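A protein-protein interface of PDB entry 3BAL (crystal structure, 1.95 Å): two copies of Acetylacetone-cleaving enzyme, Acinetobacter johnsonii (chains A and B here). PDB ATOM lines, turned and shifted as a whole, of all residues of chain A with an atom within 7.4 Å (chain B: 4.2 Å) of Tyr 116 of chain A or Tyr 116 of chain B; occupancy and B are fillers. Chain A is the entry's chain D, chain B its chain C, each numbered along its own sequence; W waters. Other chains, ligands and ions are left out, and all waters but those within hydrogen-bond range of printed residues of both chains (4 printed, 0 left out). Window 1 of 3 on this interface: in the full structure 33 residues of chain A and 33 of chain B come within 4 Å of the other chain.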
ATOM      1  N   ILE A  16      25.184 -17.506   1.806  1.00  0.00           N
ATOM      2  CA  ILE A  16      24.349 -16.337   2.017  1.00  0.00           C
ATOM      3  C   ILE A  16      24.542 -15.360   0.865  1.00  0.00           C
ATOM      4  O   ILE A  16      25.520 -14.611   0.821  1.00  0.00           O
ATOM      5  CB  ILE A  16      24.687 -15.649   3.355  1.00  0.00           C
ATOM      6  CG1 ILE A  16      24.446 -16.635   4.510  1.00  0.00           C
ATOM      7  CG2 ILE A  16      23.832 -14.399   3.527  1.00  0.00           C
ATOM      8  CD1 ILE A  16      24.864 -16.113   5.876  1.00  0.00           C
ATOM      9  N   LEU A  38      17.944 -19.497   7.504  1.00  0.00           N
ATOM     10  CA  LEU A  38      19.141 -20.305   7.261  1.00  0.00           C
ATOM     11  C   LEU A  38      19.052 -21.764   7.704  1.00  0.00           C
ATOM     12  O   LEU A  38      19.599 -22.649   7.041  1.00  0.00           O
ATOM     13  CB  LEU A  38      20.352 -19.653   7.942  1.00  0.00           C
ATOM     14  CG  LEU A  38      20.759 -18.264   7.445  1.00  0.00           C
ATOM     15  CD1 LEU A  38      21.780 -17.644   8.394  1.00  0.00           C
ATOM     16  CD2 LEU A  38      21.323 -18.375   6.036  1.00  0.00           C
ATOM     17  N   HIS A  39      18.372 -22.018   8.821  1.00  0.00           N
ATOM     18  CA  HIS A  39      18.258 -23.383   9.340  1.00  0.00           C
ATOM     19  C   HIS A  39      17.125 -23.575  10.351  1.00  0.00           C
ATOM     20  O   HIS A  39      16.840 -22.679  11.138  1.00  0.00           O
ATOM     21  CB  HIS A  39      19.599 -23.791   9.985  1.00  0.00           C
ATOM     22  CG  HIS A  39      19.568 -25.119  10.681  1.00  0.00           C
ATOM     23  ND1 HIS A  39      19.219 -25.258  12.010  1.00  0.00           N
ATOM     24  CD2 HIS A  39      19.799 -26.374  10.223  1.00  0.00           C
ATOM     25  CE1 HIS A  39      19.234 -26.539  12.336  1.00  0.00           C
ATOM     26  NE2 HIS A  39      19.582 -27.237  11.270  1.00  0.00           N
ATOM     27  N   THR A  48      17.508 -20.575  12.853  1.00  0.00           N
ATOM     28  CA  THR A  48      18.499 -19.518  12.602  1.00  0.00           C
ATOM     29  C   THR A  48      18.198 -18.701  11.334  1.00  0.00           C
ATOM     30  O   THR A  48      17.750 -19.252  10.326  1.00  0.00           O
ATOM     31  CB  THR A  48      19.904 -20.159  12.435  1.00  0.00           C
ATOM     32  OG1 THR A  48      20.213 -20.939  13.595  1.00  0.00           O
ATOM     33  CG2 THR A  48      20.975 -19.099  12.224  1.00  0.00           C
ATOM     34  N   ALA A  49      18.473 -17.399  11.382  1.00  0.00           N
ATOM     35  CA  ALA A  49      18.241 -16.527  10.234  1.00  0.00           C
ATOM     36  C   ALA A  49      19.142 -15.293  10.261  1.00  0.00           C
ATOM     37  O   ALA A  49      19.849 -15.042  11.243  1.00  0.00           O
ATOM     38  CB  ALA A  49      16.773 -16.096  10.197  1.00  0.00           C
ATOM     39  N   ILE A  50      19.114 -14.520   9.178  1.00  0.00           N
ATOM     40  CA  ILE A  50      19.911 -13.301   9.103  1.00  0.00           C
ATOM     41  C   ILE A  50      19.009 -12.183   8.559  1.00  0.00           C
ATOM     42  O   ILE A  50      18.161 -12.433   7.696  1.00  0.00           O
ATOM     43  CB  ILE A  50      21.147 -13.513   8.209  1.00  0.00           C
ATOM     44  CG1 ILE A  50      22.045 -12.276   8.273  1.00  0.00           C
ATOM     45  CG2 ILE A  50      20.718 -13.832   6.778  1.00  0.00           C
ATOM     46  CD1 ILE A  50      23.458 -12.534   7.783  1.00  0.00           C
ATOM     47  N   PHE A  51      19.176 -10.962   9.066  1.00  0.00           N
ATOM     48  CA  PHE A  51      18.327  -9.837   8.648  1.00  0.00           C
ATOM     49  C   PHE A  51      19.071  -8.568   8.211  1.00  0.00           C
ATOM     50  O   PHE A  51      20.114  -8.231   8.762  1.00  0.00           O
ATOM     51  CB  PHE A  51      17.373  -9.426   9.790  1.00  0.00           C
ATOM     52  CG  PHE A  51      16.641 -10.573  10.443  1.00  0.00           C
ATOM     53  CD1 PHE A  51      17.314 -11.455  11.295  1.00  0.00           C
ATOM     54  CD2 PHE A  51      15.277 -10.772  10.208  1.00  0.00           C
ATOM     55  CE1 PHE A  51      16.641 -12.523  11.910  1.00  0.00           C
ATOM     56  CE2 PHE A  51      14.590 -11.835  10.814  1.00  0.00           C
ATOM     57  CZ  PHE A  51      15.279 -12.716  11.669  1.00  0.00           C
ATOM     58  N   GLY A  68      17.983 -16.606  22.940  1.00  0.00           N
ATOM     59  CA  GLY A  68      18.335 -16.236  21.578  1.00  0.00           C
ATOM     60  C   GLY A  68      19.683 -15.530  21.606  1.00  0.00           C
ATOM     61  O   GLY A  68      19.969 -14.780  22.544  1.00  0.00           O
ATOM     62  N   GLU A  69      20.519 -15.763  20.597  1.00  0.00           N
ATOM     63  CA  GLU A  69      21.845 -15.138  20.535  1.00  0.00           C
ATOM     64  C   GLU A  69      22.053 -14.420  19.208  1.00  0.00           C
ATOM     65  O   GLU A  69      21.811 -15.000  18.153  1.00  0.00           O
ATOM     66  CB  GLU A  69      22.947 -16.193  20.707  1.00  0.00           C
ATOM     67  CG  GLU A  69      23.135 -16.679  22.130  1.00  0.00           C
ATOM     68  CD  GLU A  69      24.181 -17.762  22.232  1.00  0.00           C
ATOM     69  OE1 GLU A  69      23.853 -18.935  21.977  1.00  0.00           O
ATOM     70  OE2 GLU A  69      25.345 -17.437  22.550  1.00  0.00           O
ATOM     71  N   TYR A  70      22.507 -13.168  19.254  1.00  0.00           N
ATOM     72  CA  TYR A  70      22.711 -12.422  18.019  1.00  0.00           C
ATOM     73  C   TYR A  70      24.125 -11.893  17.825  1.00  0.00           C
ATOM     74  O   TYR A  70      24.871 -11.685  18.787  1.00  0.00           O
ATOM     75  CB  TYR A  70      21.715 -11.254  17.917  1.00  0.00           C
ATOM     76  CG  TYR A  70      21.954 -10.106  18.886  1.00  0.00           C
ATOM     77  CD1 TYR A  70      23.021  -9.213  18.707  1.00  0.00           C
ATOM     78  CD2 TYR A  70      21.116  -9.916  19.991  1.00  0.00           C
ATOM     79  CE1 TYR A  70      23.244  -8.163  19.612  1.00  0.00           C
ATOM     80  CE2 TYR A  70      21.332  -8.878  20.894  1.00  0.00           C
ATOM     81  CZ  TYR A  70      22.397  -8.007  20.700  1.00  0.00           C
ATOM     82  OH  TYR A  70      22.621  -6.997  21.607  1.00  0.00           O
ATOM     83  N   PHE A  71      24.469 -11.680  16.559  1.00  0.00           N
ATOM     84  CA  PHE A  71      25.764 -11.151  16.149  1.00  0.00           C
ATOM     85  C   PHE A  71      25.445  -9.980  15.204  1.00  0.00           C
ATOM     86  O   PHE A  71      25.041 -10.185  14.050  1.00  0.00           O
ATOM     87  CB  PHE A  71      26.574 -12.249  15.431  1.00  0.00           C
ATOM     88  CG  PHE A  71      27.956 -11.817  14.972  1.00  0.00           C
ATOM     89  CD1 PHE A  71      28.718 -12.656  14.157  1.00  0.00           C
ATOM     90  CD2 PHE A  71      28.481 -10.572  15.314  1.00  0.00           C
ATOM     91  CE1 PHE A  71      29.980 -12.263  13.683  1.00  0.00           C
ATOM     92  CE2 PHE A  71      29.738 -10.167  14.849  1.00  0.00           C
ATOM     93  CZ  PHE A  71      30.486 -11.016  14.030  1.00  0.00           C
ATOM     94  N   LEU A  72      25.589  -8.756  15.719  1.00  0.00           N
ATOM     95  CA  LEU A  72      25.341  -7.542  14.938  1.00  0.00           C
ATOM     96  C   LEU A  72      26.612  -7.260  14.149  1.00  0.00           C
ATOM     97  O   LEU A  72      27.634  -6.853  14.711  1.00  0.00           O
ATOM     98  CB  LEU A  72      25.021  -6.351  15.858  1.00  0.00           C
ATOM     99  CG  LEU A  72      24.707  -4.991  15.202  1.00  0.00           C
ATOM    100  CD1 LEU A  72      23.455  -5.102  14.336  1.00  0.00           C
ATOM    101  CD2 LEU A  72      24.505  -3.927  16.281  1.00  0.00           C
ATOM    102  N   THR A  73      26.531  -7.477  12.843  1.00  0.00           N
ATOM    103  CA  THR A  73      27.668  -7.298  11.946  1.00  0.00           C
ATOM    104  C   THR A  73      27.778  -5.906  11.325  1.00  0.00           C
ATOM    105  O   THR A  73      28.868  -5.487  10.931  1.00  0.00           O
ATOM    106  CB  THR A  73      27.613  -8.341  10.810  1.00  0.00           C
ATOM    107  OG1 THR A  73      26.362  -8.225  10.119  1.00  0.00           O
ATOM    108  CG2 THR A  73      27.745  -9.757  11.379  1.00  0.00           C
ATOM    109  N   SER A  94      29.170  -6.623  17.476  1.00  0.00           N
ATOM    110  CA  SER A  94      28.847  -6.952  18.862  1.00  0.00           C
ATOM    111  C   SER A  94      27.954  -8.188  18.952  1.00  0.00           C
ATOM    112  O   SER A  94      27.336  -8.611  17.972  1.00  0.00           O
ATOM    113  CB  SER A  94      28.183  -5.761  19.565  1.00  0.00           C
ATOM    114  OG  SER A  94      26.990  -5.368  18.914  1.00  0.00           O
ATOM    115  N   TYR A  95      27.896  -8.746  20.154  1.00  0.00           N
ATOM    116  CA  TYR A  95      27.140  -9.955  20.440  1.00  0.00           C
ATOM    117  C   TYR A  95      26.130  -9.704  21.555  1.00  0.00           C
ATOM    118  O   TYR A  95      26.327  -8.825  22.391  1.00  0.00           O
ATOM    119  CB  TYR A  95      28.130 -11.048  20.873  1.00  0.00           C
ATOM    120  CG  TYR A  95      27.518 -12.186  21.645  1.00  0.00           C
ATOM    121  CD1 TYR A  95      26.954 -13.280  20.987  1.00  0.00           C
ATOM    122  CD2 TYR A  95      27.455 -12.145  23.038  1.00  0.00           C
ATOM    123  CE1 TYR A  95      26.340 -14.305  21.702  1.00  0.00           C
ATOM    124  CE2 TYR A  95      26.840 -13.162  23.763  1.00  0.00           C
ATOM    125  CZ  TYR A  95      26.286 -14.237  23.089  1.00  0.00           C
ATOM    126  OH  TYR A  95      25.668 -15.234  23.809  1.00  0.00           O
ATOM    127  N   GLY A  96      25.060 -10.491  21.585  1.00  0.00           N
ATOM    128  CA  GLY A  96      24.080 -10.322  22.642  1.00  0.00           C
ATOM    129  C   GLY A  96      23.376 -11.612  23.010  1.00  0.00           C
ATOM    130  O   GLY A  96      23.118 -12.442  22.145  1.00  0.00           O
ATOM    131  N   GLN A 114      22.597  -4.917  10.068  1.00  0.00           N
ATOM    132  CA  GLN A 114      22.544  -6.331   9.732  1.00  0.00           C
ATOM    133  C   GLN A 114      22.888  -7.156  10.971  1.00  0.00           C
ATOM    134  O   GLN A 114      23.837  -6.841  11.693  1.00  0.00           O
ATOM    135  CB  GLN A 114      23.529  -6.700   8.610  1.00  0.00           C
ATOM    136  CG  GLN A 114      23.578  -8.220   8.377  1.00  0.00           C
ATOM    137  CD  GLN A 114      24.498  -8.654   7.254  1.00  0.00           C
ATOM    138  OE1 GLN A 114      24.163  -8.536   6.079  1.00  0.00           O
ATOM    139  NE2 GLN A 114      25.669  -9.159   7.615  1.00  0.00           N
ATOM    140  N   PHE A 115      22.107  -8.205  11.216  1.00  0.00           N
ATOM    141  CA  PHE A 115      22.358  -9.082  12.347  1.00  0.00           C
ATOM    142  C   PHE A 115      21.935 -10.521  12.052  1.00  0.00           C
ATOM    143  O   PHE A 115      20.956 -10.778  11.340  1.00  0.00           O
ATOM    144  CB  PHE A 115      21.679  -8.545  13.630  1.00  0.00           C
ATOM    145  CG  PHE A 115      20.176  -8.720  13.670  1.00  0.00           C
ATOM    146  CD1 PHE A 115      19.608  -9.806  14.333  1.00  0.00           C
ATOM    147  CD2 PHE A 115      19.327  -7.783  13.073  1.00  0.00           C
ATOM    148  CE1 PHE A 115      18.221  -9.955  14.410  1.00  0.00           C
ATOM    149  CE2 PHE A 115      17.938  -7.921  13.143  1.00  0.00           C
ATOM    150  CZ  PHE A 115      17.384  -9.008  13.812  1.00  0.00           C
ATOM    151  N   TYR A 116      22.737 -11.441  12.587  1.00  0.00           N
ATOM    152  CA  TYR A 116      22.562 -12.887  12.464  1.00  0.00           C
ATOM    153  C   TYR A 116      22.023 -13.319  13.824  1.00  0.00           C
ATOM    154  O   TYR A 116      22.449 -12.781  14.850  1.00  0.00           O
ATOM    155  CB  TYR A 116      23.934 -13.524  12.199  1.00  0.00           C
ATOM    156  CG  TYR A 116      24.021 -15.031  12.351  1.00  0.00           C
ATOM    157  CD1 TYR A 116      23.853 -15.882  11.256  1.00  0.00           C
ATOM    158  CD2 TYR A 116      24.328 -15.606  13.591  1.00  0.00           C
ATOM    159  CE1 TYR A 116      23.998 -17.276  11.394  1.00  0.00           C
ATOM    160  CE2 TYR A 116      24.470 -16.985  13.738  1.00  0.00           C
ATOM    161  CZ  TYR A 116      24.307 -17.816  12.638  1.00  0.00           C
ATOM    162  OH  TYR A 116      24.475 -19.178  12.792  1.00  0.00           O
ATOM    163  N   MET A 117      21.099 -14.275  13.857  1.00  0.00           N
ATOM    164  CA  MET A 117      20.553 -14.693  15.148  1.00  0.00           C
ATOM    165  C   MET A 117      20.017 -16.113  15.205  1.00  0.00           C
ATOM    166  O   MET A 117      19.382 -16.591  14.260  1.00  0.00           O
ATOM    167  CB  MET A 117      19.447 -13.722  15.579  1.00  0.00           C
ATOM    168  CG  MET A 117      18.866 -13.983  16.967  1.00  0.00           C
ATOM    169  SD  MET A 117      18.031 -12.490  17.594  1.00  0.00           S
ATOM    170  CE  MET A 117      17.917 -12.860  19.364  1.00  0.00           C
ATOM    171  N   THR A 118      20.283 -16.785  16.325  1.00  0.00           N
ATOM    172  CA  THR A 118      19.797 -18.147  16.544  1.00  0.00           C
ATOM    173  C   THR A 118      18.717 -18.077  17.632  1.00  0.00           C
ATOM    174  O   THR A 118      18.869 -17.351  18.617  1.00  0.00           O
ATOM    175  CB  THR A 118      20.946 -19.122  16.974  1.00  0.00           C
ATOM    176  OG1 THR A 118      21.677 -18.561  18.072  1.00  0.00           O
ATOM    177  CG2 THR A 118      21.904 -19.378  15.808  1.00  0.00           C
ATOM    178  N   PHE A 119      17.617 -18.806  17.436  1.00  0.00           N
ATOM    179  CA  PHE A 119      16.512 -18.812  18.394  1.00  0.00           C
ATOM    180  C   PHE A 119      16.177 -20.226  18.853  1.00  0.00           C
ATOM    181  O   PHE A 119      16.178 -21.151  18.046  1.00  0.00           O
ATOM    182  CB  PHE A 119      15.218 -18.238  17.783  1.00  0.00           C
ATOM    183  CG  PHE A 119      15.385 -16.920  17.069  1.00  0.00           C
ATOM    184  CD1 PHE A 119      15.786 -16.881  15.736  1.00  0.00           C
ATOM    185  CD2 PHE A 119      15.118 -15.719  17.723  1.00  0.00           C
ATOM    186  CE1 PHE A 119      15.916 -15.659  15.060  1.00  0.00           C
ATOM    187  CE2 PHE A 119      15.245 -14.490  17.058  1.00  0.00           C
ATOM    188  CZ  PHE A 119      15.645 -14.461  15.725  1.00  0.00           C
ATOM    189  N   LEU B  38      32.845 -15.473  23.695  1.00  0.00           N
ATOM    190  CA  LEU B  38      31.777 -14.497  23.817  1.00  0.00           C
ATOM    191  C   LEU B  38      30.704 -14.798  24.862  1.00  0.00           C
ATOM    192  O   LEU B  38      30.147 -13.872  25.454  1.00  0.00           O
ATOM    193  CB  LEU B  38      31.121 -14.300  22.448  1.00  0.00           C
ATOM    194  CG  LEU B  38      32.032 -13.724  21.363  1.00  0.00           C
ATOM    195  CD1 LEU B  38      31.340 -13.827  20.012  1.00  0.00           C
ATOM    196  CD2 LEU B  38      32.374 -12.262  21.686  1.00  0.00           C
ATOM    197  N   THR B  48      29.660 -19.819  22.996  1.00  0.00           N
ATOM    198  CA  THR B  48      29.840 -19.079  21.747  1.00  0.00           C
ATOM    199  C   THR B  48      31.177 -18.328  21.702  1.00  0.00           C
ATOM    200  O   THR B  48      31.624 -17.771  22.707  1.00  0.00           O
ATOM    201  CB  THR B  48      28.677 -18.065  21.582  1.00  0.00           C
ATOM    202  OG1 THR B  48      27.430 -18.771  21.649  1.00  0.00           O
ATOM    203  CG2 THR B  48      28.768 -17.315  20.263  1.00  0.00           C
ATOM    204  N   ALA B  49      31.804 -18.306  20.527  1.00  0.00           N
ATOM    205  CA  ALA B  49      33.094 -17.640  20.350  1.00  0.00           C
ATOM    206  C   ALA B  49      33.265 -17.132  18.916  1.00  0.00           C
ATOM    207  O   ALA B  49      32.476 -17.461  18.032  1.00  0.00           O
ATOM    208  CB  ALA B  49      34.231 -18.614  20.703  1.00  0.00           C
ATOM    209  N   GLU B  69      26.843 -24.417  15.098  1.00  0.00           N
ATOM    210  CA  GLU B  69      26.467 -23.605  13.937  1.00  0.00           C
ATOM    211  C   GLU B  69      27.475 -22.489  13.719  1.00  0.00           C
ATOM    212  O   GLU B  69      27.807 -21.762  14.650  1.00  0.00           O
ATOM    213  CB  GLU B  69      25.063 -22.998  14.123  1.00  0.00           C
ATOM    214  CG  GLU B  69      23.966 -24.043  14.282  1.00  0.00           C
ATOM    215  CD  GLU B  69      22.575 -23.456  14.396  1.00  0.00           C
ATOM    216  OE1 GLU B  69      22.007 -23.039  13.368  1.00  0.00           O
ATOM    217  OE2 GLU B  69      22.040 -23.400  15.526  1.00  0.00           O
ATOM    218  N   TYR B  70      27.963 -22.348  12.493  1.00  0.00           N
ATOM    219  CA  TYR B  70      28.938 -21.299  12.229  1.00  0.00           C
ATOM    220  C   TYR B  70      28.482 -20.272  11.198  1.00  0.00           C
ATOM    221  O   TYR B  70      27.666 -20.558  10.315  1.00  0.00           O
ATOM    222  CB  TYR B  70      30.276 -21.911  11.796  1.00  0.00           C
ATOM    223  CG  TYR B  70      30.249 -22.574  10.439  1.00  0.00           C
ATOM    224  CD1 TYR B  70      30.260 -21.816   9.268  1.00  0.00           C
ATOM    225  CD2 TYR B  70      30.203 -23.960  10.323  1.00  0.00           C
ATOM    226  CE1 TYR B  70      30.226 -22.430   8.005  1.00  0.00           C
ATOM    227  CE2 TYR B  70      30.170 -24.582   9.077  1.00  0.00           C
ATOM    228  CZ  TYR B  70      30.178 -23.817   7.924  1.00  0.00           C
ATOM    229  OH  TYR B  70      30.131 -24.439   6.694  1.00  0.00           O
ATOM    230  N   PHE B  71      29.026 -19.070  11.341  1.00  0.00           N
ATOM    231  CA  PHE B  71      28.749 -17.953  10.452  1.00  0.00           C
ATOM    232  C   PHE B  71      30.124 -17.438   9.988  1.00  0.00           C
ATOM    233  O   PHE B  71      30.839 -16.790  10.754  1.00  0.00           O
ATOM    234  CB  PHE B  71      27.983 -16.863  11.216  1.00  0.00           C
ATOM    235  CG  PHE B  71      27.643 -15.638  10.393  1.00  0.00           C
ATOM    236  CD1 PHE B  71      27.243 -14.456  11.028  1.00  0.00           C
ATOM    237  CD2 PHE B  71      27.720 -15.653   8.999  1.00  0.00           C
ATOM    238  CE1 PHE B  71      26.928 -13.308  10.288  1.00  0.00           C
ATOM    239  CE2 PHE B  71      27.408 -14.508   8.248  1.00  0.00           C
ATOM    240  CZ  PHE B  71      27.011 -13.332   8.898  1.00  0.00           C
ATOM    241  N   TYR B  95      26.833 -19.889   6.036  1.00  0.00           N
ATOM    242  CA  TYR B  95      26.414 -20.551   7.265  1.00  0.00           C
ATOM    243  C   TYR B  95      26.608 -22.060   7.175  1.00  0.00           C
ATOM    244  O   TYR B  95      26.638 -22.626   6.084  1.00  0.00           O
ATOM    245  CB  TYR B  95      24.928 -20.229   7.508  1.00  0.00           C
ATOM    246  CG  TYR B  95      24.227 -21.172   8.454  1.00  0.00           C
ATOM    247  CD1 TYR B  95      24.280 -20.976   9.836  1.00  0.00           C
ATOM    248  CD2 TYR B  95      23.551 -22.297   7.966  1.00  0.00           C
ATOM    249  CE1 TYR B  95      23.682 -21.876  10.710  1.00  0.00           C
ATOM    250  CE2 TYR B  95      22.952 -23.206   8.830  1.00  0.00           C
ATOM    251  CZ  TYR B  95      23.023 -22.992  10.205  1.00  0.00           C
ATOM    252  OH  TYR B  95      22.463 -23.911  11.067  1.00  0.00           O
ATOM    253  N   PHE B 115      35.290 -16.196  11.567  1.00  0.00           N
ATOM    254  CA  PHE B 115      34.024 -16.898  11.733  1.00  0.00           C
ATOM    255  C   PHE B 115      33.560 -16.942  13.187  1.00  0.00           C
ATOM    256  O   PHE B 115      34.362 -17.023  14.120  1.00  0.00           O
ATOM    257  CB  PHE B 115      34.110 -18.314  11.125  1.00  0.00           C
ATOM    258  CG  PHE B 115      34.792 -19.322  12.000  1.00  0.00           C
ATOM    259  CD1 PHE B 115      34.050 -20.121  12.871  1.00  0.00           C
ATOM    260  CD2 PHE B 115      36.179 -19.484  11.950  1.00  0.00           C
ATOM    261  CE1 PHE B 115      34.678 -21.071  13.683  1.00  0.00           C
ATOM    262  CE2 PHE B 115      36.821 -20.429  12.756  1.00  0.00           C
ATOM    263  CZ  PHE B 115      36.069 -21.227  13.625  1.00  0.00           C
ATOM    264  N   TYR B 116      32.242 -16.872  13.337  1.00  0.00           N
ATOM    265  CA  TYR B 116      31.519 -16.878  14.610  1.00  0.00           C
ATOM    266  C   TYR B 116      30.843 -18.247  14.721  1.00  0.00           C
ATOM    267  O   TYR B 116      30.337 -18.764  13.728  1.00  0.00           O
ATOM    268  CB  TYR B 116      30.476 -15.754  14.561  1.00  0.00           C
ATOM    269  CG  TYR B 116      29.403 -15.763  15.629  1.00  0.00           C
ATOM    270  CD1 TYR B 116      29.524 -14.978  16.775  1.00  0.00           C
ATOM    271  CD2 TYR B 116      28.229 -16.505  15.458  1.00  0.00           C
ATOM    272  CE1 TYR B 116      28.494 -14.925  17.716  1.00  0.00           C
ATOM    273  CE2 TYR B 116      27.202 -16.458  16.396  1.00  0.00           C
ATOM    274  CZ  TYR B 116      27.336 -15.670  17.516  1.00  0.00           C
ATOM    275  OH  TYR B 116      26.312 -15.618  18.433  1.00  0.00           O
ATOM    276  N   MET B 117      30.829 -18.833  15.916  1.00  0.00           N
ATOM    277  CA  MET B 117      30.226 -20.151  16.090  1.00  0.00           C
ATOM    278  C   MET B 117      29.676 -20.417  17.482  1.00  0.00           C
ATOM    279  O   MET B 117      30.247 -19.985  18.485  1.00  0.00           O
ATOM    280  CB  MET B 117      31.257 -21.232  15.745  1.00  0.00           C
ATOM    281  CG  MET B 117      30.737 -22.670  15.727  1.00  0.00           C
ATOM    282  SD  MET B 117      31.923 -23.731  14.837  1.00  0.00           S
ATOM    283  CE  MET B 117      30.883 -25.227  14.482  1.00  0.00           C
ATOM    284  N   THR B 118      28.563 -21.144  17.532  1.00  0.00           N
ATOM    285  CA  THR B 118      27.924 -21.524  18.796  1.00  0.00           C
ATOM    286  C   THR B 118      28.046 -23.050  18.912  1.00  0.00           C
ATOM    287  O   THR B 118      27.822 -23.761  17.929  1.00  0.00           O
ATOM    288  CB  THR B 118      26.429 -21.107  18.809  1.00  0.00           C
ATOM    289  OG1 THR B 118      25.764 -21.651  17.659  1.00  0.00           O
ATOM    290  CG2 THR B 118      26.298 -19.586  18.784  1.00  0.00           C
HETATM  291  O   HOH W   1      25.669 -20.895  22.684  1.00  0.00           O
HETATM  292  O   HOH W   2      19.502 -22.420  16.125  1.00  0.00           O
HETATM  293  O   HOH W   3      24.012 -16.678  17.410  1.00  0.00           O
HETATM  294  O   HOH W   4      25.851 -19.649  15.129  1.00  0.00           O
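OE2 of Glu 69 of chain A is in hydrogen-bond range of OG1 of Thr 48 of chain B. The side-chain carboxylate of Glu 69 of chain B sits at hydrogen-bond distance from the side-chain hydroxyl of Thr 48 of chain A (2.8 Å).
OE1 of Glu 69 of chain B touches ND1 of His 39 of chain A, 3.8 Å away. His 39 of chain A touches Tyr 95 of chain B. Ile 50 of chain A touches Phe 71 of chain B. CD1 of Phe 71 of chain A touches CD1 of Phe 71 of chain B (3.9 Å). Tyr 116 of chain B touches Phe 71 of chain A. Thr 73 of chain A touches Phe 71 of chain B (CG2 to CE1, 3.8 Å). Leu 38 of chain B touches Tyr 95 of chain A. OH of Tyr 116 of chain B touches CD1 of Tyr 95 of chain A (3.5 Å). CG of Tyr 116 of chain A touches CD1 of Phe 71 of chain B, 3.5 Å away. Tyr 116 of chain A touches Tyr 95 of chain B (OH to CD1, 3.5 Å).
Thr 48 of chain A touches Glu 69 of chain B, and with the chains exchanged Glu 69 of chain A touches Thr 48 of chain B. Phe 71 of chain A touches Tyr 116 of chain B, and with the chains exchanged Tyr 116 of chain A touches Phe 71 of chain B. Tyr 95 of chain A touches Tyr 116 of chain B, and with the chains exchanged Tyr 116 of chain A touches Tyr 95 of chain B. Tyr 116 of chain B touches its own counterpart, Tyr 116 of chain A. Of the 15 pairs that touch across the chains among the printed residues, 10 have their exchanged pair printed and touching as well.
The backbone carbonyl oxygen (O) of Thr 48 of chain B sits at hydrogen-bond distance from the backbone NH (N) of Leu 38 of chain B (2.8 Å). The side-chain carboxylate (OE1) of Glu 69 of chain B is in hydrogen-bond range of the side-chain hydroxyl (OH) of Tyr 95 of chain B (2.5 Å). The backbone carbonyl oxygen (O) of Thr 48 of chain A is in hydrogen-bond range of the backbone NH (N) of Leu 38 of chain A (2.8 Å). OE2 of Glu 69 of chain A sits at hydrogen-bond distance from OH of Tyr 95 of chain A. O of Tyr 116 of chain A lies within hydrogen-bond range of N of Phe 71 of chain A. The side-chain hydroxyl (OG1) of Thr 73 of chain A lies within hydrogen-bond range of the side-chain amide nitrogen (NE2) of Gln 114 of chain A (2.8 Å).
Tyr 116 of chain A touches just these residues of chain B: Phe 71, Tyr 95 and Tyr 116. Tyr 116 of chain B touches just these residues of chain A: Phe 71 (3.5 Å), Tyr 95 (3.5 Å) and Tyr 116 (3.8 Å). Printed residues of chain B within 4 Å of Glu 69 of chain A: Thr 48 (2.6 Å). Of the printed residues of chain B, Ile 50 of chain A touches Phe 71. The nearest residue of chain B that does not touch Tyr 116 of chain A is Glu 69 of chain B (4.1 Å). The nearest residue of chain A that does not touch Tyr 116 of chain B is Glu 69 of chain A (4.1 Å).
Of the 11 printed residues of chain B, 6 touch a printed residue of chain A. Printed residues of chain B that touch a printed residue of chain A: Leu 38, Thr 48, Glu 69, Phe 71, Tyr 95 and Tyr 116. Hydrophobic or aromatic side chains of chain B within 4 Å of the printed part of chain A: Phe 71, Tyr 95 and Tyr 116.
Water W3 lies within hydrogen-bond range of OH of Tyr 116 of chain B (2.7 Å), O of Glu 69 of chain A (2.9 Å) and OG1 of Thr 118 of chain A (3.1 Å). Water W4 lies within hydrogen-bond range of the side-chain hydroxyl (OH) of Tyr 116 of chain A (2.8 Å), the backbone carbonyl oxygen (O) of Glu 69 of chain B (2.9 Å) and the side-chain hydroxyl (OG1) of Thr 118 of chain B (3.2 Å). Water W1 bridges the side-chain carboxylate (OE1) of Glu 69 of chain A (2.8 Å) and the side-chain hydroxyl (OG1) of Thr 48 of chain B (2.9 Å). Water W2 bridges OE2 of Glu 69 of chain B (2.8 Å) and OG1 of Thr 48 of chain A (3.0 Å).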
